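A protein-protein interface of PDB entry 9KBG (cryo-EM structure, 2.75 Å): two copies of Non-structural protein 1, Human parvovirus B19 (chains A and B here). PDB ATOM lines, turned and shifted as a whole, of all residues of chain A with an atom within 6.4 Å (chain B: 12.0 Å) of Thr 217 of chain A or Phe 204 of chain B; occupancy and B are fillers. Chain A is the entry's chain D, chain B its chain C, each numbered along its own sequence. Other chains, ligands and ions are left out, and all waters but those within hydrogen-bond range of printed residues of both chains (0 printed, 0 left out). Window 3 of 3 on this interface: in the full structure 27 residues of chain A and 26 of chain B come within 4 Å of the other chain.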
ATOM      1  N   SER A 212     -17.023 -25.713  17.160  1.00  0.00           N
ATOM      2  CA  SER A 212     -18.477 -25.731  17.288  1.00  0.00           C
ATOM      3  C   SER A 212     -18.936 -26.836  18.233  1.00  0.00           C
ATOM      4  O   SER A 212     -19.861 -26.638  19.030  1.00  0.00           O
ATOM      5  CB  SER A 212     -19.121 -25.895  15.913  1.00  0.00           C
ATOM      6  OG  SER A 212     -18.442 -26.872  15.146  1.00  0.00           O
ATOM      7  N   ILE A 213     -18.301 -28.007  18.159  1.00  0.00           N
ATOM      8  CA  ILE A 213     -18.649 -29.103  19.060  1.00  0.00           C
ATOM      9  C   ILE A 213     -18.333 -28.727  20.502  1.00  0.00           C
ATOM     10  O   ILE A 213     -19.116 -29.005  21.419  1.00  0.00           O
ATOM     11  CB  ILE A 213     -17.927 -30.393  18.632  1.00  0.00           C
ATOM     12  CG1 ILE A 213     -18.503 -30.908  17.312  1.00  0.00           C
ATOM     13  CG2 ILE A 213     -18.043 -31.459  19.708  1.00  0.00           C
ATOM     14  CD1 ILE A 213     -17.596 -31.871  16.585  1.00  0.00           C
ATOM     15  N   LYS A 214     -17.180 -28.090  20.726  1.00  0.00           N
ATOM     16  CA  LYS A 214     -16.831 -27.649  22.072  1.00  0.00           C
ATOM     17  C   LYS A 214     -17.815 -26.602  22.584  1.00  0.00           C
ATOM     18  O   LYS A 214     -18.186 -26.610  23.764  1.00  0.00           O
ATOM     19  CB  LYS A 214     -15.404 -27.105  22.092  1.00  0.00           C
ATOM     20  CG  LYS A 214     -14.901 -26.732  23.473  1.00  0.00           C
ATOM     21  CD  LYS A 214     -13.491 -26.174  23.415  1.00  0.00           C
ATOM     22  CE  LYS A 214     -13.038 -25.680  24.779  1.00  0.00           C
ATOM     23  NZ  LYS A 214     -11.682 -25.068  24.729  1.00  0.00           N
ATOM     24  N   PHE A 215     -18.244 -25.688  21.711  1.00  0.00           N
ATOM     25  CA  PHE A 215     -19.230 -24.685  22.103  1.00  0.00           C
ATOM     26  C   PHE A 215     -20.558 -25.334  22.476  1.00  0.00           C
ATOM     27  O   PHE A 215     -21.201 -24.934  23.453  1.00  0.00           O
ATOM     28  CB  PHE A 215     -19.419 -23.675  20.971  1.00  0.00           C
ATOM     29  CG  PHE A 215     -20.378 -22.565  21.293  1.00  0.00           C
ATOM     30  CD1 PHE A 215     -20.000 -21.522  22.119  1.00  0.00           C
ATOM     31  CD2 PHE A 215     -21.656 -22.561  20.760  1.00  0.00           C
ATOM     32  CE1 PHE A 215     -20.877 -20.501  22.412  1.00  0.00           C
ATOM     33  CE2 PHE A 215     -22.538 -21.541  21.051  1.00  0.00           C
ATOM     34  CZ  PHE A 215     -22.149 -20.510  21.877  1.00  0.00           C
ATOM     35  N   GLN A 216     -20.985 -26.340  21.708  1.00  0.00           N
ATOM     36  CA  GLN A 216     -22.217 -27.051  22.037  1.00  0.00           C
ATOM     37  C   GLN A 216     -22.093 -27.786  23.367  1.00  0.00           C
ATOM     38  O   GLN A 216     -23.033 -27.797  24.173  1.00  0.00           O
ATOM     39  CB  GLN A 216     -22.573 -28.027  20.916  1.00  0.00           C
ATOM     40  CG  GLN A 216     -23.966 -28.621  21.031  1.00  0.00           C
ATOM     41  CD  GLN A 216     -24.372 -29.394  19.793  1.00  0.00           C
ATOM     42  OE1 GLN A 216     -23.525 -29.900  19.058  1.00  0.00           O
ATOM     43  NE2 GLN A 216     -25.675 -29.488  19.556  1.00  0.00           N
ATOM     44  N   THR A 217     -20.938 -28.409  23.613  1.00  0.00           N
ATOM     45  CA  THR A 217     -20.711 -29.076  24.891  1.00  0.00           C
ATOM     46  C   THR A 217     -20.760 -28.081  26.045  1.00  0.00           C
ATOM     47  O   THR A 217     -21.322 -28.374  27.106  1.00  0.00           O
ATOM     48  CB  THR A 217     -19.368 -29.807  24.872  1.00  0.00           C
ATOM     49  OG1 THR A 217     -19.356 -30.758  23.801  1.00  0.00           O
ATOM     50  CG2 THR A 217     -19.138 -30.536  26.186  1.00  0.00           C
ATOM     51  N   MET A 218     -20.176 -26.896  25.854  1.00  0.00           N
ATOM     52  CA  MET A 218     -20.220 -25.872  26.893  1.00  0.00           C
ATOM     53  C   MET A 218     -21.644 -25.383  27.132  1.00  0.00           C
ATOM     54  O   MET A 218     -22.030 -25.116  28.274  1.00  0.00           O
ATOM     55  CB  MET A 218     -19.301 -24.710  26.519  1.00  0.00           C
ATOM     56  CG  MET A 218     -19.175 -23.645  27.593  1.00  0.00           C
ATOM     57  SD  MET A 218     -17.895 -22.436  27.207  1.00  0.00           S
ATOM     58  CE  MET A 218     -18.738 -21.425  25.995  1.00  0.00           C
ATOM     59  N   VAL A 219     -22.437 -25.256  26.065  1.00  0.00           N
ATOM     60  CA  VAL A 219     -23.837 -24.864  26.222  1.00  0.00           C
ATOM     61  C   VAL A 219     -24.596 -25.912  27.026  1.00  0.00           C
ATOM     62  O   VAL A 219     -25.385 -25.584  27.923  1.00  0.00           O
ATOM     63  CB  VAL A 219     -24.482 -24.629  24.842  1.00  0.00           C
ATOM     64  CG1 VAL A 219     -25.999 -24.624  24.952  1.00  0.00           C
ATOM     65  CG2 VAL A 219     -23.984 -23.327  24.239  1.00  0.00           C
ATOM     66  N   ASN A 220     -24.367 -27.192  26.720  1.00  0.00           N
ATOM     67  CA  ASN A 220     -25.021 -28.259  27.472  1.00  0.00           C
ATOM     68  C   ASN A 220     -24.595 -28.244  28.935  1.00  0.00           C
ATOM     69  O   ASN A 220     -25.425 -28.431  29.834  1.00  0.00           O
ATOM     70  CB  ASN A 220     -24.713 -29.614  26.836  1.00  0.00           C
ATOM     71  CG  ASN A 220     -25.526 -29.865  25.584  1.00  0.00           C
ATOM     72  OD1 ASN A 220     -26.632 -29.349  25.436  1.00  0.00           O
ATOM     73  ND2 ASN A 220     -24.978 -30.661  24.674  1.00  0.00           N
ATOM     74  N   TRP A 221     -23.303 -28.020  29.191  1.00  0.00           N
ATOM     75  CA  TRP A 221     -22.817 -27.929  30.564  1.00  0.00           C
ATOM     76  C   TRP A 221     -23.471 -26.774  31.307  1.00  0.00           C
ATOM     77  O   TRP A 221     -23.843 -26.909  32.479  1.00  0.00           O
ATOM     78  CB  TRP A 221     -21.294 -27.778  30.567  1.00  0.00           C
ATOM     79  CG  TRP A 221     -20.685 -27.712  31.935  1.00  0.00           C
ATOM     80  CD1 TRP A 221     -20.166 -28.750  32.650  1.00  0.00           C
ATOM     81  CD2 TRP A 221     -20.512 -26.542  32.745  1.00  0.00           C
ATOM     82  NE1 TRP A 221     -19.692 -28.303  33.858  1.00  0.00           N
ATOM     83  CE2 TRP A 221     -19.892 -26.950  33.940  1.00  0.00           C
ATOM     84  CE3 TRP A 221     -20.827 -25.190  32.577  1.00  0.00           C
ATOM     85  CZ2 TRP A 221     -19.580 -26.057  34.962  1.00  0.00           C
ATOM     86  CZ3 TRP A 221     -20.518 -24.305  33.592  1.00  0.00           C
ATOM     87  CH2 TRP A 221     -19.901 -24.742  34.768  1.00  0.00           C
ATOM     88  N   LEU A 222     -23.612 -25.624  30.644  1.00  0.00           N
ATOM     89  CA  LEU A 222     -24.282 -24.486  31.264  1.00  0.00           C
ATOM     90  C   LEU A 222     -25.735 -24.812  31.576  1.00  0.00           C
ATOM     91  O   LEU A 222     -26.259 -24.414  32.622  1.00  0.00           O
ATOM     92  CB  LEU A 222     -24.197 -23.264  30.349  1.00  0.00           C
ATOM     93  CG  LEU A 222     -22.923 -22.419  30.397  1.00  0.00           C
ATOM     94  CD1 LEU A 222     -23.029 -21.261  29.421  1.00  0.00           C
ATOM     95  CD2 LEU A 222     -22.660 -21.915  31.805  1.00  0.00           C
ATOM     96  N   ASP A 237     -17.515 -21.255  38.263  1.00  0.00           N
ATOM     97  CA  ASP A 237     -16.331 -21.624  37.485  1.00  0.00           C
ATOM     98  C   ASP A 237     -15.587 -20.354  37.077  1.00  0.00           C
ATOM     99  O   ASP A 237     -15.856 -19.779  36.019  1.00  0.00           O
ATOM    100  CB  ASP A 237     -16.725 -22.460  36.269  1.00  0.00           C
ATOM    101  CG  ASP A 237     -15.595 -23.340  35.776  1.00  0.00           C
ATOM    102  OD1 ASP A 237     -14.480 -23.244  36.328  1.00  0.00           O
ATOM    103  OD2 ASP A 237     -15.821 -24.129  34.836  1.00  0.00           O
ATOM    104  N   GLN A 240     -12.719 -21.236  33.874  1.00  0.00           N
ATOM    105  CA  GLN A 240     -13.181 -21.221  32.491  1.00  0.00           C
ATOM    106  C   GLN A 240     -13.608 -19.824  32.064  1.00  0.00           C
ATOM    107  O   GLN A 240     -13.397 -19.431  30.911  1.00  0.00           O
ATOM    108  CB  GLN A 240     -14.326 -22.216  32.307  1.00  0.00           C
ATOM    109  CG  GLN A 240     -14.701 -22.467  30.854  1.00  0.00           C
ATOM    110  CD  GLN A 240     -13.601 -23.157  30.072  1.00  0.00           C
ATOM    111  OE1 GLN A 240     -12.750 -23.839  30.643  1.00  0.00           O
ATOM    112  NE2 GLN A 240     -13.612 -22.981  28.756  1.00  0.00           N
ATOM    113  N   VAL B 201     -21.218 -29.497  41.412  1.00  0.00           N
ATOM    114  CA  VAL B 201     -20.462 -28.542  40.613  1.00  0.00           C
ATOM    115  C   VAL B 201     -19.132 -29.150  40.183  1.00  0.00           C
ATOM    116  O   VAL B 201     -18.288 -29.482  41.016  1.00  0.00           O
ATOM    117  CB  VAL B 201     -20.239 -27.227  41.383  1.00  0.00           C
ATOM    118  CG1 VAL B 201     -19.128 -26.415  40.740  1.00  0.00           C
ATOM    119  CG2 VAL B 201     -21.528 -26.423  41.440  1.00  0.00           C
ATOM    120  N   VAL B 202     -18.957 -29.305  38.875  1.00  0.00           N
ATOM    121  CA  VAL B 202     -17.720 -29.842  38.310  1.00  0.00           C
ATOM    122  C   VAL B 202     -17.198 -28.855  37.273  1.00  0.00           C
ATOM    123  O   VAL B 202     -17.953 -28.437  36.383  1.00  0.00           O
ATOM    124  CB  VAL B 202     -17.936 -31.233  37.694  1.00  0.00           C
ATOM    125  CG1 VAL B 202     -16.615 -31.809  37.213  1.00  0.00           C
ATOM    126  CG2 VAL B 202     -18.593 -32.167  38.698  1.00  0.00           C
ATOM    127  N   PRO B 203     -15.932 -28.446  37.354  1.00  0.00           N
ATOM    128  CA  PRO B 203     -15.397 -27.503  36.365  1.00  0.00           C
ATOM    129  C   PRO B 203     -15.437 -28.079  34.956  1.00  0.00           C
ATOM    130  O   PRO B 203     -15.267 -29.283  34.750  1.00  0.00           O
ATOM    131  CB  PRO B 203     -13.956 -27.275  36.838  1.00  0.00           C
ATOM    132  CG  PRO B 203     -13.985 -27.597  38.295  1.00  0.00           C
ATOM    133  CD  PRO B 203     -14.968 -28.721  38.433  1.00  0.00           C
ATOM    134  N   PHE B 204     -15.674 -27.200  33.984  1.00  0.00           N
ATOM    135  CA  PHE B 204     -15.706 -27.612  32.588  1.00  0.00           C
ATOM    136  C   PHE B 204     -14.339 -28.124  32.154  1.00  0.00           C
ATOM    137  O   PHE B 204     -13.300 -27.612  32.580  1.00  0.00           O
ATOM    138  CB  PHE B 204     -16.145 -26.443  31.705  1.00  0.00           C
ATOM    139  CG  PHE B 204     -16.427 -26.829  30.280  1.00  0.00           C
ATOM    140  CD1 PHE B 204     -17.352 -27.816  29.986  1.00  0.00           C
ATOM    141  CD2 PHE B 204     -15.769 -26.201  29.237  1.00  0.00           C
ATOM    142  CE1 PHE B 204     -17.613 -28.170  28.677  1.00  0.00           C
ATOM    143  CE2 PHE B 204     -16.027 -26.551  27.925  1.00  0.00           C
ATOM    144  CZ  PHE B 204     -16.950 -27.537  27.645  1.00  0.00           C
ATOM    145  N   ASN B 205     -14.343 -29.141  31.295  1.00  0.00           N
ATOM    146  CA  ASN B 205     -13.118 -29.803  30.864  1.00  0.00           C
ATOM    147  C   ASN B 205     -12.357 -29.027  29.795  1.00  0.00           C
ATOM    148  O   ASN B 205     -11.382 -29.554  29.250  1.00  0.00           O
ATOM    149  CB  ASN B 205     -13.435 -31.211  30.352  1.00  0.00           C
ATOM    150  CG  ASN B 205     -13.487 -32.238  31.465  1.00  0.00           C
ATOM    151  OD1 ASN B 205     -12.634 -32.252  32.352  1.00  0.00           O
ATOM    152  ND2 ASN B 205     -14.492 -33.104  31.424  1.00  0.00           N
ATOM    153  N   GLY B 206     -12.779 -27.805  29.479  1.00  0.00           N
ATOM    154  CA  GLY B 206     -12.045 -27.012  28.508  1.00  0.00           C
ATOM    155  C   GLY B 206     -10.643 -26.694  28.998  1.00  0.00           C
ATOM    156  O   GLY B 206     -10.437 -26.309  30.151  1.00  0.00           O
ATOM    157  N   LYS B 207      -9.670 -26.857  28.105  1.00  0.00           N
ATOM    158  CA  LYS B 207      -8.270 -26.599  28.408  1.00  0.00           C
ATOM    159  C   LYS B 207      -7.779 -25.432  27.564  1.00  0.00           C
ATOM    160  O   LYS B 207      -8.043 -25.369  26.359  1.00  0.00           O
ATOM    161  CB  LYS B 207      -7.408 -27.841  28.148  1.00  0.00           C
ATOM    162  CG  LYS B 207      -5.962 -27.700  28.593  1.00  0.00           C
ATOM    163  CD  LYS B 207      -5.867 -27.549  30.104  1.00  0.00           C
ATOM    164  CE  LYS B 207      -4.438 -27.281  30.549  1.00  0.00           C
ATOM    165  NZ  LYS B 207      -3.542 -28.442  30.284  1.00  0.00           N
ATOM    166  N   GLY B 208      -7.062 -24.509  28.204  1.00  0.00           N
ATOM    167  CA  GLY B 208      -6.636 -23.300  27.537  1.00  0.00           C
ATOM    168  C   GLY B 208      -5.354 -23.461  26.741  1.00  0.00           C
ATOM    169  O   GLY B 208      -4.681 -24.488  26.791  1.00  0.00           O
ATOM    170  N   THR B 209      -5.028 -22.409  25.997  1.00  0.00           N
ATOM    171  CA  THR B 209      -3.824 -22.365  25.183  1.00  0.00           C
ATOM    172  C   THR B 209      -2.732 -21.602  25.931  1.00  0.00           C
ATOM    173  O   THR B 209      -2.881 -21.254  27.105  1.00  0.00           O
ATOM    174  CB  THR B 209      -4.132 -21.736  23.826  1.00  0.00           C
ATOM    175  OG1 THR B 209      -4.464 -20.355  24.003  1.00  0.00           O
ATOM    176  CG2 THR B 209      -5.302 -22.447  23.167  1.00  0.00           C
ATOM    177  N   SER B 212      -4.022 -17.988  26.825  1.00  0.00           N
ATOM    178  CA  SER B 212      -4.974 -17.926  27.930  1.00  0.00           C
ATOM    179  C   SER B 212      -4.270 -18.062  29.274  1.00  0.00           C
ATOM    180  O   SER B 212      -4.645 -17.400  30.250  1.00  0.00           O
ATOM    181  CB  SER B 212      -6.037 -19.011  27.767  1.00  0.00           C
ATOM    182  OG  SER B 212      -6.799 -18.805  26.593  1.00  0.00           O
ATOM    183  N   GLN B 216      -4.335 -15.485  32.438  1.00  0.00           N
ATOM    184  CA  GLN B 216      -4.643 -15.863  33.816  1.00  0.00           C
ATOM    185  C   GLN B 216      -3.515 -15.471  34.764  1.00  0.00           C
ATOM    186  O   GLN B 216      -3.765 -14.987  35.875  1.00  0.00           O
ATOM    187  CB  GLN B 216      -4.916 -17.364  33.894  1.00  0.00           C
ATOM    188  CG  GLN B 216      -5.555 -17.814  35.193  1.00  0.00           C
ATOM    189  CD  GLN B 216      -6.060 -19.240  35.124  1.00  0.00           C
ATOM    190  OE1 GLN B 216      -5.466 -20.088  34.458  1.00  0.00           O
ATOM    191  NE2 GLN B 216      -7.164 -19.512  35.808  1.00  0.00           N
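Among the printed residues, merely in contact across the chains: Lys 214 of chain A with Lys 207 of chain B (3.999 Å), Thr 217 of chain A with Phe 204 of chain B (3.8 Å), Met 218 of chain A with Phe 204 of chain B (3.7 Å), Trp 221 of chain A with Phe 204 of chain B (3.9 Å), Asp 237 of chain A with Pro 203 of chain B (3.7 Å) and Gln 240 of chain A with Phe 204 of chain B (3.8 Å).
Ile 213 of chain A touches none of the printed residues of chain B. Of the printed residues of chain B, Lys 214 of chain A touches Lys 207. No residue of chain B comes within 4 Å of Gln 216 of chain A. Thr 217 of chain A touches one residue of chain B. Met 218 of chain A touches just one residue of chain B: Phe 204 (3.7 Å). No residue of chain B comes within 4 Å of Val 219 of chain A. Of chain B, only Phe 204 and Gly 206 come within 4 Å of Gln 240 of chain A. Phe 204 of chain B touches just these residues of chain A: Thr 217, Met 218, Trp 221, Asp 237 and Gln 240. Printed residues of chain A within 4 Å of Gly 206 of chain B: Gln 240. Of the printed residues of chain A, Lys 207 of chain B touches Lys 214 (3.999 Å). Gln 216 of chain B touches none of the printed residues of chain A. The nearest residue of chain A that does not touch Phe 204 of chain B is Lys 214 of chain A (4.2 Å). The nearest printed residue of chain A that does not touch Gly 206 of chain B is Lys 214 of chain A (4.1 Å).
Positions printed for both chains: 212 and 216. Of the 9 pairs that touch across the chains among the printed residues, none has its exchanged pair printed and touching as well.
Printed residues of chain B that touch a printed residue of chain A: Val 202, Pro 203, Phe 204, Gly 206 and Lys 207. Hydrophobic or aromatic side chains of chain A within 4 Å of the printed part of chain B: Met 218 and Trp 221.
OG1 of Thr 217 of chain A lies within hydrogen-bond range of O of Ile 213 of chain A (3.0 Å).
NE1 of Trp 221 of chain A sits at hydrogen-bond distance from O of Val 202 of chain B (3.1 Å). N of Phe 204 of chain B lies within hydrogen-bond range of OD2 of Asp 237 of chain A (3.2 Å). The side-chain amide oxygen of Gln 240 of chain A lies close to the backbone carbonyl oxygen of Gly 206 of chain B (3.4 Å).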
